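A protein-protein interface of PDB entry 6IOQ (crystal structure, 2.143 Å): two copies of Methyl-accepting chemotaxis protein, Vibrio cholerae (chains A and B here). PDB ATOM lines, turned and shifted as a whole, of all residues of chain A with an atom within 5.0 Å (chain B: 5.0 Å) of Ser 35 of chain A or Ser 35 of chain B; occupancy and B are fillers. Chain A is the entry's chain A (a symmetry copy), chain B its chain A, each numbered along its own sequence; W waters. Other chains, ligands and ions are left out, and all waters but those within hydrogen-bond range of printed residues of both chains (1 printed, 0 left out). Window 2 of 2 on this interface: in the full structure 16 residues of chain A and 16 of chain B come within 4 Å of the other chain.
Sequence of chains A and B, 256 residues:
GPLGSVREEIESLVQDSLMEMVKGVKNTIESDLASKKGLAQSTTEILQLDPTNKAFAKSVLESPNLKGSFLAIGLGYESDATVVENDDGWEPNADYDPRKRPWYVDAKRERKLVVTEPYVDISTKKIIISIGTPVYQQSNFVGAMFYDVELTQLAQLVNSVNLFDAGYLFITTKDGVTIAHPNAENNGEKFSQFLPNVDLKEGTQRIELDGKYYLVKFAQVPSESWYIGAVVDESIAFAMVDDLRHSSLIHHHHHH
OG of Ser 31 of chain B sits at hydrogen-bond distance from OG of Ser 31 of chain A (3.2 Å).
The backbone carbonyl oxygen (O) of Ser 31 of chain A sits at hydrogen-bond distance from the side-chain hydroxyl (OG) of Ser 35 of chain A. The backbone carbonyl oxygen of Asp 32 of chain A lies within hydrogen-bond range of the side-chain hydroxyl of Ser 35 of chain A. The side-chain hydroxyl of Ser 35 of chain B is in hydrogen-bond range of the backbone carbonyl oxygen of Asp 32 of chain B (3.0 Å). OG of Ser 35 of chain B sits at hydrogen-bond distance from O of Ser 31 of chain B.
Among the printed residues, merely in contact across the chains: Ser 35 of chain A with Ser 35 of chain B, Gly 38 of chain A with Leu 39 of chain B and Leu 39 of chain A with Gly 38 of chain B.
Of the printed residues of chain B, Ser 31 of chain A touches Ser 31 (3.2 Å). Of the printed residues of chain B, Ser 35 of chain A touches Ser 35 (3.5 Å). Of the printed residues of chain B, Gly 38 of chain A touches Leu 39. Of the printed residues of chain A, Ser 31 of chain B touches Ser 31. Ser 35 of chain B touches just one residue of chain A: Ser 35 (3.5 Å). The nearest printed residue of chain B that does not touch Ser 35 of chain A is Ser 31 of chain B (5.6 Å). The nearest printed residue of chain A that does not touch Ser 35 of chain B is Ser 31 of chain A (5.6 Å). The nearest printed residue of chain A that does not touch Leu 39 of chain B is Leu 39 of chain A (4.03 Å).
Of the 10 printed residues of chain B, 4 touch a printed residue of chain A. Printed residues of chain B that touch a printed residue of chain A: Ser 31, Ser 35, Gly 38 and Leu 39. Hydrophobic or aromatic side chains of chain B that line the printed part of chain A: Leu 39. Printed residues of chain A that touch a printed residue of chain B: Ser 31, Ser 35, Gly 38 and Leu 39. Hydrophobic or aromatic side chains of chain A within 4 Å of the printed part of chain B: Leu 39. Among the printed residues, 4 pairs touch across the chains.
Ser 31 of chain B touches its own counterpart, Ser 31 of chain A. Ser 35 of chain A touches its own counterpart, Ser 35 of chain B. Gly 38 of chain A touches Leu 39 of chain B, and with the chains exchanged Leu 39 of chain A touches Gly 38 of chain B. Of the 4 pairs that touch across the chains among the printed residues, 4 have their exchanged pair printed and touching as well.
Water W1 bridges the side-chain hydroxyl (OG) of Ser 31 of chain A (2.9 Å) and the side-chain hydroxyl (OG) of Ser 31 of chain B (2.9 Å).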
ATOM      1  N   GLU A  30      17.635 -14.205 -18.391  1.00  0.00           N
ATOM      2  CA  GLU A  30      17.919 -12.779 -18.353  1.00  0.00           C
ATOM      3  C   GLU A  30      18.828 -12.415 -17.189  1.00  0.00           C
ATOM      4  O   GLU A  30      19.780 -11.648 -17.352  1.00  0.00           O
ATOM      5  CB  GLU A  30      16.630 -11.976 -18.247  1.00  0.00           C
ATOM      6  CG  GLU A  30      15.858 -11.886 -19.525  1.00  0.00           C
ATOM      7  CD  GLU A  30      14.582 -11.072 -19.387  1.00  0.00           C
ATOM      8  OE1 GLU A  30      14.161 -10.779 -18.243  1.00  0.00           O
ATOM      9  OE2 GLU A  30      14.003 -10.722 -20.439  1.00  0.00           O
ATOM     10  N   SER A  31      18.514 -12.955 -16.015  1.00  0.00           N
ATOM     11  CA  SER A  31      19.327 -12.751 -14.820  1.00  0.00           C
ATOM     12  C   SER A  31      20.735 -13.319 -14.959  1.00  0.00           C
ATOM     13  O   SER A  31      21.700 -12.694 -14.543  1.00  0.00           O
ATOM     14  CB  SER A  31      18.649 -13.380 -13.592  1.00  0.00           C
ATOM     15  OG  SER A  31      17.478 -12.654 -13.240  1.00  0.00           O
ATOM     16  N   ASP A  32      20.867 -14.506 -15.526  1.00  0.00           N
ATOM     17  CA  ASP A  32      22.212 -15.054 -15.683  1.00  0.00           C
ATOM     18  C   ASP A  32      23.032 -14.219 -16.665  1.00  0.00           C
ATOM     19  O   ASP A  32      24.181 -13.894 -16.417  1.00  0.00           O
ATOM     20  CB  ASP A  32      22.176 -16.496 -16.154  1.00  0.00           C
ATOM     21  CG  ASP A  32      23.564 -17.132 -16.153  1.00  0.00           C
ATOM     22  OD1 ASP A  32      24.004 -17.574 -15.067  1.00  0.00           O
ATOM     23  OD2 ASP A  32      24.211 -17.213 -17.221  1.00  0.00           O
ATOM     24  N   LEU A  33      22.422 -13.869 -17.785  1.00  0.00           N
ATOM     25  CA  LEU A  33      23.079 -13.068 -18.802  1.00  0.00           C
ATOM     26  C   LEU A  33      23.511 -11.698 -18.257  1.00  0.00           C
ATOM     27  O   LEU A  33      24.672 -11.312 -18.375  1.00  0.00           O
ATOM     28  CB  LEU A  33      22.137 -12.913 -19.991  1.00  0.00           C
ATOM     29  CG  LEU A  33      22.674 -12.323 -21.287  1.00  0.00           C
ATOM     30  CD1 LEU A  33      23.959 -13.021 -21.702  1.00  0.00           C
ATOM     31  CD2 LEU A  33      21.605 -12.457 -22.355  1.00  0.00           C
ATOM     32  N   ALA A  34      22.576 -10.972 -17.635  1.00  0.00           N
ATOM     33  CA  ALA A  34      22.891  -9.671 -17.045  1.00  0.00           C
ATOM     34  C   ALA A  34      24.032  -9.760 -16.036  1.00  0.00           C
ATOM     35  O   ALA A  34      24.887  -8.884 -16.008  1.00  0.00           O
ATOM     36  CB  ALA A  34      21.650  -9.061 -16.378  1.00  0.00           C
ATOM     37  N   SER A  35      24.061 -10.794 -15.196  1.00  0.00           N
ATOM     38  CA  SER A  35      25.136 -10.864 -14.220  1.00  0.00           C
ATOM     39  C   SER A  35      26.472 -11.187 -14.910  1.00  0.00           C
ATOM     40  O   SER A  35      27.527 -10.665 -14.518  1.00  0.00           O
ATOM     41  CB  SER A  35      24.822 -11.882 -13.128  1.00  0.00           C
ATOM     42  OG  SER A  35      24.891 -13.194 -13.623  1.00  0.00           O
ATOM     43  N   LYS A  36      26.431 -12.021 -15.950  1.00  0.00           N
ATOM     44  CA  LYS A  36      27.635 -12.305 -16.741  1.00  0.00           C
ATOM     45  C   LYS A  36      28.123 -11.048 -17.457  1.00  0.00           C
ATOM     46  O   LYS A  36      29.317 -10.778 -17.507  1.00  0.00           O
ATOM     47  CB  LYS A  36      27.371 -13.420 -17.770  1.00  0.00           C
ATOM     48  CG  LYS A  36      27.442 -14.849 -17.209  1.00  0.00           C
ATOM     49  CD  LYS A  36      27.116 -15.883 -18.293  1.00  0.00           C
ATOM     50  CE  LYS A  36      27.460 -17.321 -17.874  1.00  0.00           C
ATOM     51  NZ  LYS A  36      26.611 -17.787 -16.758  1.00  0.00           N
ATOM     52  N   LYS A  37      27.197 -10.289 -18.024  1.00  0.00           N
ATOM     53  CA  LYS A  37      27.555  -9.043 -18.708  1.00  0.00           C
ATOM     54  C   LYS A  37      28.155  -8.016 -17.751  1.00  0.00           C
ATOM     55  O   LYS A  37      29.105  -7.333 -18.097  1.00  0.00           O
ATOM     56  CB  LYS A  37      26.336  -8.419 -19.393  1.00  0.00           C
ATOM     57  CG  LYS A  37      25.891  -9.130 -20.651  1.00  0.00           C
ATOM     58  CD  LYS A  37      24.693  -8.427 -21.257  1.00  0.00           C
ATOM     59  CE  LYS A  37      24.232  -9.091 -22.542  1.00  0.00           C
ATOM     60  NZ  LYS A  37      23.047  -8.369 -23.087  1.00  0.00           N
ATOM     61  N   GLY A  38      27.561  -7.885 -16.569  1.00  0.00           N
ATOM     62  CA  GLY A  38      28.067  -6.975 -15.547  1.00  0.00           C
ATOM     63  C   GLY A  38      29.487  -7.315 -15.126  1.00  0.00           C
ATOM     64  O   GLY A  38      30.320  -6.447 -14.973  1.00  0.00           O
ATOM     65  N   LEU A  39      29.772  -8.600 -14.955  1.00  0.00           N
ATOM     66  CA  LEU A  39      31.111  -9.067 -14.620  1.00  0.00           C
ATOM     67  C   LEU A  39      32.124  -8.769 -15.733  1.00  0.00           C
ATOM     68  O   LEU A  39      33.257  -8.318 -15.473  1.00  0.00           O
ATOM     69  CB  LEU A  39      31.051 -10.585 -14.346  1.00  0.00           C
ATOM     70  CG  LEU A  39      31.890 -11.248 -13.262  1.00  0.00           C
ATOM     71  CD1 LEU A  39      31.606 -10.648 -11.902  1.00  0.00           C
ATOM     72  CD2 LEU A  39      31.604 -12.746 -13.217  1.00  0.00           C
ATOM     73  N   GLU B  30      16.853 -12.862  -5.240  1.00  0.00           N
ATOM     74  CA  GLU B  30      17.959 -13.807  -5.244  1.00  0.00           C
ATOM     75  C   GLU B  30      18.947 -13.514  -6.363  1.00  0.00           C
ATOM     76  O   GLU B  30      20.161 -13.530  -6.148  1.00  0.00           O
ATOM     77  CB  GLU B  30      17.448 -15.233  -5.394  1.00  0.00           C
ATOM     78  CG  GLU B  30      16.842 -15.800  -4.149  1.00  0.00           C
ATOM     79  CD  GLU B  30      16.350 -17.226  -4.330  1.00  0.00           C
ATOM     80  OE1 GLU B  30      16.249 -17.699  -5.486  1.00  0.00           O
ATOM     81  OE2 GLU B  30      16.066 -17.875  -3.299  1.00  0.00           O
ATOM     82  N   SER B  31      18.417 -13.266  -7.557  1.00  0.00           N
ATOM     83  CA  SER B  31      19.233 -12.906  -8.713  1.00  0.00           C
ATOM     84  C   SER B  31      19.982 -11.591  -8.522  1.00  0.00           C
ATOM     85  O   SER B  31      21.143 -11.480  -8.887  1.00  0.00           O
ATOM     86  CB  SER B  31      18.365 -12.812  -9.978  1.00  0.00           C
ATOM     87  OG  SER B  31      17.909 -14.101 -10.370  1.00  0.00           O
ATOM     88  N   ASP B  32      19.327 -10.585  -7.968  1.00  0.00           N
ATOM     89  CA  ASP B  32      20.038  -9.326  -7.761  1.00  0.00           C
ATOM     90  C   ASP B  32      21.155  -9.490  -6.732  1.00  0.00           C
ATOM     91  O   ASP B  32      22.269  -9.031  -6.926  1.00  0.00           O
ATOM     92  CB  ASP B  32      19.098  -8.221  -7.314  1.00  0.00           C
ATOM     93  CG  ASP B  32      19.794  -6.863  -7.265  1.00  0.00           C
ATOM     94  OD1 ASP B  32      19.914  -6.228  -8.336  1.00  0.00           O
ATOM     95  OD2 ASP B  32      20.206  -6.416  -6.170  1.00  0.00           O
ATOM     96  N   LEU B  33      20.844 -10.159  -5.635  1.00  0.00           N
ATOM     97  CA  LEU B  33      21.812 -10.397  -4.578  1.00  0.00           C
ATOM     98  C   LEU B  33      23.020 -11.199  -5.084  1.00  0.00           C
ATOM     99  O   LEU B  33      24.166 -10.786  -4.910  1.00  0.00           O
ATOM    100  CB  LEU B  33      21.116 -11.119  -3.429  1.00  0.00           C
ATOM    101  CG  LEU B  33      21.847 -11.270  -2.102  1.00  0.00           C
ATOM    102  CD1 LEU B  33      22.406  -9.934  -1.642  1.00  0.00           C
ATOM    103  CD2 LEU B  33      20.879 -11.842  -1.083  1.00  0.00           C
ATOM    104  N   ALA B  34      22.762 -12.338  -5.735  1.00  0.00           N
ATOM    105  CA  ALA B  34      23.838 -13.157  -6.291  1.00  0.00           C
ATOM    106  C   ALA B  34      24.723 -12.367  -7.251  1.00  0.00           C
ATOM    107  O   ALA B  34      25.937 -12.527  -7.229  1.00  0.00           O
ATOM    108  CB  ALA B  34      23.271 -14.394  -7.001  1.00  0.00           C
ATOM    109  N   SER B  35      24.142 -11.524  -8.104  1.00  0.00           N
ATOM    110  CA  SER B  35      24.985 -10.790  -9.034  1.00  0.00           C
ATOM    111  C   SER B  35      25.805  -9.721  -8.292  1.00  0.00           C
ATOM    112  O   SER B  35      26.972  -9.473  -8.630  1.00  0.00           O
ATOM    113  CB  SER B  35      24.157 -10.168 -10.153  1.00  0.00           C
ATOM    114  OG  SER B  35      23.379  -9.101  -9.676  1.00  0.00           O
ATOM    115  N   LYS B  36      25.213  -9.106  -7.267  1.00  0.00           N
ATOM    116  CA  LYS B  36      25.947  -8.150  -6.429  1.00  0.00           C
ATOM    117  C   LYS B  36      27.077  -8.847  -5.675  1.00  0.00           C
ATOM    118  O   LYS B  36      28.179  -8.322  -5.569  1.00  0.00           O
ATOM    119  CB  LYS B  36      25.007  -7.452  -5.429  1.00  0.00           C
ATOM    120  CG  LYS B  36      24.204  -6.277  -6.009  1.00  0.00           C
ATOM    121  CD  LYS B  36      23.262  -5.682  -4.955  1.00  0.00           C
ATOM    122  CE  LYS B  36      22.662  -4.333  -5.380  1.00  0.00           C
ATOM    123  NZ  LYS B  36      21.755  -4.474  -6.538  1.00  0.00           N
ATOM    124  N   LYS B  37      26.795 -10.024  -5.137  1.00  0.00           N
ATOM    125  CA  LYS B  37      27.817 -10.793  -4.419  1.00  0.00           C
ATOM    126  C   LYS B  37      28.963 -11.215  -5.335  1.00  0.00           C
ATOM    127  O   LYS B  37      30.117 -11.170  -4.938  1.00  0.00           O
ATOM    128  CB  LYS B  37      27.216 -12.047  -3.778  1.00  0.00           C
ATOM    129  CG  LYS B  37      26.373 -11.782  -2.552  1.00  0.00           C
ATOM    130  CD  LYS B  37      25.840 -13.084  -1.987  1.00  0.00           C
ATOM    131  CE  LYS B  37      25.014 -12.866  -0.733  1.00  0.00           C
ATOM    132  NZ  LYS B  37      24.506 -14.174  -0.229  1.00  0.00           N
ATOM    133  N   GLY B  38      28.629 -11.667  -6.539  1.00  0.00           N
ATOM    134  CA  GLY B  38      29.632 -12.055  -7.525  1.00  0.00           C
ATOM    135  C   GLY B  38      30.555 -10.904  -7.889  1.00  0.00           C
ATOM    136  O   GLY B  38      31.752 -11.069  -7.993  1.00  0.00           O
ATOM    137  N   LEU B  39      29.992  -9.715  -8.067  1.00  0.00           N
ATOM    138  CA  LEU B  39      30.768  -8.516  -8.351  1.00  0.00           C
ATOM    139  C   LEU B  39      31.701  -8.140  -7.191  1.00  0.00           C
ATOM    140  O   LEU B  39      32.879  -7.791  -7.395  1.00  0.00           O
ATOM    141  CB  LEU B  39      29.796  -7.355  -8.650  1.00  0.00           C
ATOM    142  CG  LEU B  39      30.091  -6.299  -9.706  1.00  0.00           C
ATOM    143  CD1 LEU B  39      30.297  -6.926 -11.068  1.00  0.00           C
ATOM    144  CD2 LEU B  39      28.943  -5.298  -9.785  1.00  0.00           C
HETATM  145  O   HOH W   1      15.471 -14.148 -11.859  1.00  0.00           O
